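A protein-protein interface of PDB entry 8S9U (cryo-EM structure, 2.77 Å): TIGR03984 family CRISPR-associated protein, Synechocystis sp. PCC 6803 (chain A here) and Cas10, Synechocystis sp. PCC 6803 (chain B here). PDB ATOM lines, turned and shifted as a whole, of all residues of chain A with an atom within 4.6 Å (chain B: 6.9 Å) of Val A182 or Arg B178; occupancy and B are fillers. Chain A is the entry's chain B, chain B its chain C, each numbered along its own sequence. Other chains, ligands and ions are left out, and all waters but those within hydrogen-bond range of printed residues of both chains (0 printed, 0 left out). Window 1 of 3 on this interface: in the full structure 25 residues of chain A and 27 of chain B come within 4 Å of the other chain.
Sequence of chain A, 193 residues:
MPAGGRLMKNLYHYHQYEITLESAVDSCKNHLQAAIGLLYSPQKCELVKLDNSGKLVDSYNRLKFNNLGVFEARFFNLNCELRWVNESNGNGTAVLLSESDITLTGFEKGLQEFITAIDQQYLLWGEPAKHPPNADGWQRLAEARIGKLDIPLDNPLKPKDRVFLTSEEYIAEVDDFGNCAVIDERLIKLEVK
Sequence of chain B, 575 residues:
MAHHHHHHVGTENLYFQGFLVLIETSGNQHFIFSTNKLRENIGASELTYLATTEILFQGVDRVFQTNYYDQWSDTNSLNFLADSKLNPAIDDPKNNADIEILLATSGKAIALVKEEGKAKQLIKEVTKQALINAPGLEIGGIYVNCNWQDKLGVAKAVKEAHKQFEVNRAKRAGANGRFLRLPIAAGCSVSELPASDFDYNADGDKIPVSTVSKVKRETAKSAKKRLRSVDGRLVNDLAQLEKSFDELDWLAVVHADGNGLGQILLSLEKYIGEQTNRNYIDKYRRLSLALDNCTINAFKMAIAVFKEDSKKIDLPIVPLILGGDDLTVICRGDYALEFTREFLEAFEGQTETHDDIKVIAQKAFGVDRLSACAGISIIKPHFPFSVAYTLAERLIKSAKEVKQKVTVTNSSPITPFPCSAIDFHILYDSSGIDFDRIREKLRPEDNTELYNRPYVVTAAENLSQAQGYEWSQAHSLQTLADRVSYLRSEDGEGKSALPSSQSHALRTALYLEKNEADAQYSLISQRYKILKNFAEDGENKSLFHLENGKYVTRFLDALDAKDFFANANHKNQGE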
ATOM      1  N   ILE A 118      -8.724  -5.070  12.040  1.00  0.00           N
ATOM      2  CA  ILE A 118      -9.901  -4.769  11.236  1.00  0.00           C
ATOM      3  C   ILE A 118      -9.613  -3.526  10.410  1.00  0.00           C
ATOM      4  O   ILE A 118      -9.107  -2.528  10.932  1.00  0.00           O
ATOM      5  CB  ILE A 118     -11.162  -4.587  12.100  1.00  0.00           C
ATOM      6  CG1 ILE A 118     -11.015  -3.424  13.072  1.00  0.00           C
ATOM      7  CG2 ILE A 118     -11.445  -5.852  12.882  1.00  0.00           C
ATOM      8  CD1 ILE A 118     -12.284  -3.110  13.815  1.00  0.00           C
ATOM      9  N   GLN A 120     -10.265  -0.115   8.361  1.00  0.00           N
ATOM     10  CA  GLN A 120     -11.143   1.044   8.351  1.00  0.00           C
ATOM     11  C   GLN A 120     -10.784   1.959   7.194  1.00  0.00           C
ATOM     12  O   GLN A 120      -9.740   1.824   6.561  1.00  0.00           O
ATOM     13  CB  GLN A 120     -11.066   1.834   9.663  1.00  0.00           C
ATOM     14  CG  GLN A 120     -11.424   1.057  10.906  1.00  0.00           C
ATOM     15  CD  GLN A 120     -12.859   0.547  10.912  1.00  0.00           C
ATOM     16  OE1 GLN A 120     -13.664   0.895  10.051  1.00  0.00           O
ATOM     17  NE2 GLN A 120     -13.179  -0.283  11.892  1.00  0.00           N
ATOM     18  N   GLU A 169      -7.029  -1.361  12.512  1.00  0.00           N
ATOM     19  CA  GLU A 169      -7.097  -1.263  13.958  1.00  0.00           C
ATOM     20  C   GLU A 169      -6.800  -2.621  14.560  1.00  0.00           C
ATOM     21  O   GLU A 169      -7.322  -3.635  14.100  1.00  0.00           O
ATOM     22  CB  GLU A 169      -8.479  -0.818  14.420  1.00  0.00           C
ATOM     23  CG  GLU A 169      -8.940   0.493  13.878  1.00  0.00           C
ATOM     24  CD  GLU A 169     -10.355   0.800  14.294  1.00  0.00           C
ATOM     25  OE1 GLU A 169     -11.281   0.137  13.795  1.00  0.00           O
ATOM     26  OE2 GLU A 169     -10.546   1.707  15.126  1.00  0.00           O
ATOM     27  N   TYR A 170      -5.980  -2.642  15.597  1.00  0.00           N
ATOM     28  CA  TYR A 170      -5.562  -3.885  16.222  1.00  0.00           C
ATOM     29  C   TYR A 170      -6.262  -4.028  17.562  1.00  0.00           C
ATOM     30  O   TYR A 170      -6.085  -3.195  18.453  1.00  0.00           O
ATOM     31  CB  TYR A 170      -4.048  -3.929  16.383  1.00  0.00           C
ATOM     32  CG  TYR A 170      -3.326  -3.603  15.106  1.00  0.00           C
ATOM     33  CD1 TYR A 170      -3.035  -2.299  14.767  1.00  0.00           C
ATOM     34  CD2 TYR A 170      -2.961  -4.604  14.224  1.00  0.00           C
ATOM     35  CE1 TYR A 170      -2.399  -1.999  13.601  1.00  0.00           C
ATOM     36  CE2 TYR A 170      -2.314  -4.311  13.055  1.00  0.00           C
ATOM     37  CZ  TYR A 170      -2.038  -3.007  12.750  1.00  0.00           C
ATOM     38  OH  TYR A 170      -1.383  -2.701  11.586  1.00  0.00           O
ATOM     39  N   ILE A 171      -7.078  -5.060  17.682  1.00  0.00           N
ATOM     40  CA  ILE A 171      -7.804  -5.358  18.905  1.00  0.00           C
ATOM     41  C   ILE A 171      -6.928  -6.231  19.793  1.00  0.00           C
ATOM     42  O   ILE A 171      -6.332  -7.205  19.322  1.00  0.00           O
ATOM     43  CB  ILE A 171      -9.142  -6.039  18.584  1.00  0.00           C
ATOM     44  CG1 ILE A 171     -10.047  -5.056  17.848  1.00  0.00           C
ATOM     45  CG2 ILE A 171      -9.816  -6.528  19.841  1.00  0.00           C
ATOM     46  CD1 ILE A 171     -11.344  -5.643  17.402  1.00  0.00           C
ATOM     47  N   ALA A 181      -9.993  -4.040  23.516  1.00  0.00           N
ATOM     48  CA  ALA A 181     -10.084  -2.699  22.957  1.00  0.00           C
ATOM     49  C   ALA A 181      -9.171  -2.629  21.747  1.00  0.00           C
ATOM     50  O   ALA A 181      -8.304  -3.483  21.560  1.00  0.00           O
ATOM     51  CB  ALA A 181      -9.707  -1.624  23.980  1.00  0.00           C
ATOM     52  N   VAL A 182      -9.377  -1.610  20.916  1.00  0.00           N
ATOM     53  CA  VAL A 182      -8.453  -1.339  19.820  1.00  0.00           C
ATOM     54  C   VAL A 182      -7.224  -0.627  20.381  1.00  0.00           C
ATOM     55  O   VAL A 182      -7.275   0.542  20.765  1.00  0.00           O
ATOM     56  CB  VAL A 182      -9.126  -0.546  18.694  1.00  0.00           C
ATOM     57  CG1 VAL A 182     -10.277  -1.338  18.151  1.00  0.00           C
ATOM     58  CG2 VAL A 182      -9.683   0.751  19.196  1.00  0.00           C
ATOM     59  N   ILE A 183      -6.111  -1.355  20.457  1.00  0.00           N
ATOM     60  CA  ILE A 183      -4.900  -0.808  21.051  1.00  0.00           C
ATOM     61  C   ILE A 183      -4.145   0.123  20.117  1.00  0.00           C
ATOM     62  O   ILE A 183      -3.355   0.945  20.593  1.00  0.00           O
ATOM     63  CB  ILE A 183      -3.978  -1.938  21.527  1.00  0.00           C
ATOM     64  CG1 ILE A 183      -3.728  -2.931  20.401  1.00  0.00           C
ATOM     65  CG2 ILE A 183      -4.579  -2.627  22.723  1.00  0.00           C
ATOM     66  CD1 ILE A 183      -2.492  -3.752  20.575  1.00  0.00           C
ATOM     67  N   ASP A 184      -4.358   0.030  18.810  1.00  0.00           N
ATOM     68  CA  ASP A 184      -3.742   0.979  17.897  1.00  0.00           C
ATOM     69  C   ASP A 184      -4.523   0.996  16.596  1.00  0.00           C
ATOM     70  O   ASP A 184      -5.386   0.155  16.356  1.00  0.00           O
ATOM     71  CB  ASP A 184      -2.275   0.633  17.650  1.00  0.00           C
ATOM     72  CG  ASP A 184      -1.470   1.828  17.210  1.00  0.00           C
ATOM     73  OD1 ASP A 184      -1.442   2.113  15.998  1.00  0.00           O
ATOM     74  OD2 ASP A 184      -0.875   2.493  18.079  1.00  0.00           O
ATOM     75  N   ALA B 130     -18.385  -6.802  20.047  1.00  0.00           N
ATOM     76  CA  ALA B 130     -18.899  -5.436  20.044  1.00  0.00           C
ATOM     77  C   ALA B 130     -17.996  -4.484  19.274  1.00  0.00           C
ATOM     78  O   ALA B 130     -18.485  -3.595  18.569  1.00  0.00           O
ATOM     79  CB  ALA B 130     -19.086  -4.945  21.471  1.00  0.00           C
ATOM     80  N   LEU B 131     -16.677  -4.624  19.419  1.00  0.00           N
ATOM     81  CA  LEU B 131     -15.764  -3.773  18.662  1.00  0.00           C
ATOM     82  C   LEU B 131     -15.911  -3.992  17.167  1.00  0.00           C
ATOM     83  O   LEU B 131     -15.828  -3.044  16.380  1.00  0.00           O
ATOM     84  CB  LEU B 131     -14.324  -4.037  19.082  1.00  0.00           C
ATOM     85  CG  LEU B 131     -13.916  -3.471  20.431  1.00  0.00           C
ATOM     86  CD1 LEU B 131     -12.587  -4.038  20.821  1.00  0.00           C
ATOM     87  CD2 LEU B 131     -13.855  -1.970  20.344  1.00  0.00           C
ATOM     88  N   ILE B 132     -16.153  -5.231  16.756  1.00  0.00           N
ATOM     89  CA  ILE B 132     -16.235  -5.541  15.339  1.00  0.00           C
ATOM     90  C   ILE B 132     -17.581  -5.121  14.774  1.00  0.00           C
ATOM     91  O   ILE B 132     -17.655  -4.383  13.787  1.00  0.00           O
ATOM     92  CB  ILE B 132     -15.974  -7.040  15.122  1.00  0.00           C
ATOM     93  CG1 ILE B 132     -14.575  -7.404  15.603  1.00  0.00           C
ATOM     94  CG2 ILE B 132     -16.135  -7.396  13.665  1.00  0.00           C
ATOM     95  CD1 ILE B 132     -14.330  -8.879  15.681  1.00  0.00           C
ATOM     96  N   ALA B 134     -20.254  -3.550  16.367  1.00  0.00           N
ATOM     97  CA  ALA B 134     -20.981  -2.453  17.009  1.00  0.00           C
ATOM     98  C   ALA B 134     -20.029  -1.317  17.361  1.00  0.00           C
ATOM     99  O   ALA B 134     -19.867  -0.967  18.530  1.00  0.00           O
ATOM    100  CB  ALA B 134     -21.714  -2.951  18.252  1.00  0.00           C
ATOM    101  N   PRO B 135     -19.354  -0.740  16.369  1.00  0.00           N
ATOM    102  CA  PRO B 135     -18.367   0.300  16.669  1.00  0.00           C
ATOM    103  C   PRO B 135     -18.995   1.471  17.409  1.00  0.00           C
ATOM    104  O   PRO B 135     -20.142   1.843  17.161  1.00  0.00           O
ATOM    105  CB  PRO B 135     -17.862   0.716  15.285  1.00  0.00           C
ATOM    106  CG  PRO B 135     -18.925   0.331  14.364  1.00  0.00           C
ATOM    107  CD  PRO B 135     -19.554  -0.891  14.921  1.00  0.00           C
ATOM    108  N   GLY B 136     -18.225   2.057  18.322  1.00  0.00           N
ATOM    109  CA  GLY B 136     -18.721   3.114  19.173  1.00  0.00           C
ATOM    110  C   GLY B 136     -19.496   2.672  20.393  1.00  0.00           C
ATOM    111  O   GLY B 136     -19.774   3.506  21.260  1.00  0.00           O
ATOM    112  N   LEU B 137     -19.889   1.408  20.481  1.00  0.00           N
ATOM    113  CA  LEU B 137     -20.567   0.902  21.665  1.00  0.00           C
ATOM    114  C   LEU B 137     -19.562   0.687  22.785  1.00  0.00           C
ATOM    115  O   LEU B 137     -18.643  -0.124  22.647  1.00  0.00           O
ATOM    116  CB  LEU B 137     -21.295  -0.396  21.345  1.00  0.00           C
ATOM    117  CG  LEU B 137     -22.169  -0.961  22.454  1.00  0.00           C
ATOM    118  CD1 LEU B 137     -23.563  -0.412  22.356  1.00  0.00           C
ATOM    119  CD2 LEU B 137     -22.187  -2.446  22.345  1.00  0.00           C
ATOM    120  N   ALA B 173      -9.876   1.448  28.765  1.00  0.00           N
ATOM    121  CA  ALA B 173      -9.829   2.349  27.618  1.00  0.00           C
ATOM    122  C   ALA B 173     -11.230   2.698  27.124  1.00  0.00           C
ATOM    123  O   ALA B 173     -12.111   1.838  27.039  1.00  0.00           O
ATOM    124  CB  ALA B 173      -9.018   1.722  26.487  1.00  0.00           C
ATOM    125  N   GLY B 174     -11.429   3.975  26.794  1.00  0.00           N
ATOM    126  CA  GLY B 174     -12.736   4.470  26.410  1.00  0.00           C
ATOM    127  C   GLY B 174     -13.038   4.300  24.929  1.00  0.00           C
ATOM    128  O   GLY B 174     -12.149   4.322  24.086  1.00  0.00           O
ATOM    129  N   ALA B 175     -14.324   4.107  24.627  1.00  0.00           N
ATOM    130  CA  ALA B 175     -14.762   3.813  23.268  1.00  0.00           C
ATOM    131  C   ALA B 175     -14.667   5.003  22.325  1.00  0.00           C
ATOM    132  O   ALA B 175     -14.842   4.821  21.115  1.00  0.00           O
ATOM    133  CB  ALA B 175     -16.200   3.294  23.283  1.00  0.00           C
ATOM    134  N   ASN B 176     -14.419   6.208  22.836  1.00  0.00           N
ATOM    135  CA  ASN B 176     -14.132   7.361  21.991  1.00  0.00           C
ATOM    136  C   ASN B 176     -12.688   7.404  21.513  1.00  0.00           C
ATOM    137  O   ASN B 176     -12.349   8.259  20.690  1.00  0.00           O
ATOM    138  CB  ASN B 176     -14.508   8.655  22.717  1.00  0.00           C
ATOM    139  CG  ASN B 176     -13.771   8.837  24.024  1.00  0.00           C
ATOM    140  OD1 ASN B 176     -12.880   8.067  24.368  1.00  0.00           O
ATOM    141  ND2 ASN B 176     -14.176   9.843  24.783  1.00  0.00           N
ATOM    142  N   GLY B 177     -11.833   6.523  22.012  1.00  0.00           N
ATOM    143  CA  GLY B 177     -10.446   6.488  21.599  1.00  0.00           C
ATOM    144  C   GLY B 177     -10.196   5.788  20.280  1.00  0.00           C
ATOM    145  O   GLY B 177      -9.088   5.307  20.035  1.00  0.00           O
ATOM    146  N   ARG B 178     -11.209   5.715  19.419  1.00  0.00           N
ATOM    147  CA  ARG B 178     -11.042   5.150  18.090  1.00  0.00           C
ATOM    148  C   ARG B 178     -11.858   5.954  17.093  1.00  0.00           C
ATOM    149  O   ARG B 178     -12.753   6.710  17.469  1.00  0.00           O
ATOM    150  CB  ARG B 178     -11.439   3.676  18.045  1.00  0.00           C
ATOM    151  CG  ARG B 178     -12.899   3.409  18.244  1.00  0.00           C
ATOM    152  CD  ARG B 178     -13.139   1.929  18.276  1.00  0.00           C
ATOM    153  NE  ARG B 178     -12.941   1.320  16.969  1.00  0.00           N
ATOM    154  CZ  ARG B 178     -13.665   0.310  16.504  1.00  0.00           C
ATOM    155  NH1 ARG B 178     -14.644  -0.190  17.237  1.00  0.00           N
ATOM    156  NH2 ARG B 178     -13.426  -0.189  15.304  1.00  0.00           N
ATOM    157  N   PHE B 179     -11.539   5.766  15.812  1.00  0.00           N
ATOM    158  CA  PHE B 179     -11.978   6.662  14.739  1.00  0.00           C
ATOM    159  C   PHE B 179     -11.494   8.078  14.993  1.00  0.00           C
ATOM    160  O   PHE B 179     -12.238   9.043  14.829  1.00  0.00           O
ATOM    161  CB  PHE B 179     -13.492   6.643  14.527  1.00  0.00           C
ATOM    162  CG  PHE B 179     -14.076   5.276  14.474  1.00  0.00           C
ATOM    163  CD1 PHE B 179     -13.823   4.456  13.402  1.00  0.00           C
ATOM    164  CD2 PHE B 179     -14.875   4.812  15.491  1.00  0.00           C
ATOM    165  CE1 PHE B 179     -14.346   3.204  13.350  1.00  0.00           C
ATOM    166  CE2 PHE B 179     -15.399   3.558  15.443  1.00  0.00           C
ATOM    167  CZ  PHE B 179     -15.136   2.751  14.373  1.00  0.00           C
ATOM    168  N   LEU B 180     -10.238   8.205  15.401  1.00  0.00           N
ATOM    169  CA  LEU B 180      -9.685   9.524  15.641  1.00  0.00           C
ATOM    170  C   LEU B 180      -9.574  10.280  14.333  1.00  0.00           C
ATOM    171  O   LEU B 180      -9.160   9.734  13.311  1.00  0.00           O
ATOM    172  CB  LEU B 180      -8.321   9.432  16.313  1.00  0.00           C
ATOM    173  CG  LEU B 180      -8.320   9.449  17.838  1.00  0.00           C
ATOM    174  CD1 LEU B 180      -8.873   8.175  18.374  1.00  0.00           C
ATOM    175  CD2 LEU B 180      -6.924   9.667  18.351  1.00  0.00           C
ATOM    176  N   ARG B 181      -9.957  11.543  14.375  1.00  0.00           N
ATOM    177  CA  ARG B 181      -9.892  12.384  13.198  1.00  0.00           C
ATOM    178  C   ARG B 181      -8.464  12.723  12.812  1.00  0.00           C
ATOM    179  O   ARG B 181      -7.590  12.907  13.661  1.00  0.00           O
ATOM    180  CB  ARG B 181     -10.680  13.670  13.427  1.00  0.00           C
ATOM    181  CG  ARG B 181     -10.680  14.618  12.246  1.00  0.00           C
ATOM    182  CD  ARG B 181     -11.763  14.306  11.256  1.00  0.00           C
ATOM    183  NE  ARG B 181     -12.991  15.028  11.520  1.00  0.00           N
ATOM    184  CZ  ARG B 181     -13.511  15.914  10.691  1.00  0.00           C
ATOM    185  NH1 ARG B 181     -12.907  16.169   9.551  1.00  0.00           N
ATOM    186  NH2 ARG B 181     -14.637  16.533  10.991  1.00  0.00           N
ATOM    187  N   LEU B 193     -17.640  12.580  14.414  1.00  0.00           N
ATOM    188  CA  LEU B 193     -16.604  11.697  13.931  1.00  0.00           C
ATOM    189  C   LEU B 193     -16.219  12.027  12.491  1.00  0.00           C
ATOM    190  O   LEU B 193     -16.951  12.723  11.790  1.00  0.00           O
ATOM    191  CB  LEU B 193     -17.084  10.261  14.035  1.00  0.00           C
ATOM    192  CG  LEU B 193     -17.358   9.796  15.450  1.00  0.00           C
ATOM    193  CD1 LEU B 193     -17.890   8.410  15.394  1.00  0.00           C
ATOM    194  CD2 LEU B 193     -16.119   9.832  16.261  1.00  0.00           C
ATOM    195  N   PRO B 194     -15.054  11.571  12.040  1.00  0.00           N
ATOM    196  CA  PRO B 194     -14.739  11.678  10.617  1.00  0.00           C
ATOM    197  C   PRO B 194     -15.682  10.818   9.797  1.00  0.00           C
ATOM    198  O   PRO B 194     -16.262   9.847  10.284  1.00  0.00           O
ATOM    199  CB  PRO B 194     -13.306  11.157  10.542  1.00  0.00           C
ATOM    200  CG  PRO B 194     -13.226  10.193  11.632  1.00  0.00           C
ATOM    201  CD  PRO B 194     -14.025  10.792  12.748  1.00  0.00           C
ATOM    202  N   THR B 211     -18.465   5.319  10.479  1.00  0.00           N
ATOM    203  CA  THR B 211     -18.733   3.895  10.608  1.00  0.00           C
ATOM    204  C   THR B 211     -19.659   3.623  11.780  1.00  0.00           C
ATOM    205  O   THR B 211     -20.429   2.660  11.753  1.00  0.00           O
ATOM    206  CB  THR B 211     -17.428   3.126  10.792  1.00  0.00           C
ATOM    207  OG1 THR B 211     -16.511   3.487   9.759  1.00  0.00           O
ATOM    208  CG2 THR B 211     -17.665   1.643  10.747  1.00  0.00           C
ATOM    209  N   VAL B 212     -19.606   4.468  12.804  1.00  0.00           N
ATOM    210  CA  VAL B 212     -20.582   4.421  13.887  1.00  0.00           C
ATOM    211  C   VAL B 212     -21.995   4.653  13.365  1.00  0.00           C
ATOM    212  O   VAL B 212     -22.884   3.814  13.537  1.00  0.00           O
ATOM    213  CB  VAL B 212     -20.202   5.432  14.980  1.00  0.00           C
ATOM    214  CG1 VAL B 212     -21.222   5.430  16.079  1.00  0.00           C
ATOM    215  CG2 VAL B 212     -18.851   5.063  15.536  1.00  0.00           C
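The backbone NH (N) of Glu A169 is in hydrogen-bond range of the backbone carbonyl oxygen (O) of Ile A118, 2.9 Å away. The side-chain amide nitrogen of Gln A120 is in hydrogen-bond range of the side-chain carboxylate of Glu A169 (2.7 Å). The guanidinium group of Arg B178 is in hydrogen-bond range of the backbone carbonyl oxygen of Leu B131, at 3.2 Å.
NH2 of Arg B178 touches CD1 of Ile A118, 3.5 Å away. Phe B179 touches Gln A120 (CE1 to CD, 3.9 Å). Gln A120 touches Thr B211. Ile A171 touches Leu B131 (CD1 to CB, 3.8 Å). Ala A181 touches Leu B131. Val A182 touches Arg B178 (CG2 to CB, 3.6 Å).
NE2 of Gln A120 lies close to NH2 of Arg B178 (3.4 Å). OE1 of Glu A169 is in salt-bridge range of NH2 of Arg B178 (2.6 Å).
Of the 20 printed residues of chain B, 4 touch a printed residue of chain A. Hydrophobic or aromatic side chains of chain B that line the printed part of chain A: Leu B131 and Phe B179. Among the printed residues, 8 pairs touch across the chains.
Of chain B, only Arg B178 (3.6 Å) comes within 4 Å of Val A182. Arg B178 touches just these residues of chain A: Ile A118 (3.5 Å), Gln A120 (3.4 Å), Glu A169 (2.6 Å) and Val A182 (3.6 Å). Of the printed residues of chain A, Leu B131 touches Ile A171 (3.8 Å) and Ala A181 (3.6 Å). Of the printed residues of chain B, Ala A181 touches Leu B131 (3.6 Å). Printed residues of chain B within 4 Å of Ile A118: Arg B178. Of the printed residues of chain B, Ile A171 touches Leu B131 (3.8 Å). Of the printed residues of chain B, Glu A169 touches Arg B178 (2.6 Å). Gly B136 touches none of the printed residues of chain A. The nearest residue of chain B that does not touch Val A182 is Leu B131 (4.03 Å). The nearest printed residue of chain A that does not touch Arg B178 is Ile A171 (6.2 Å).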
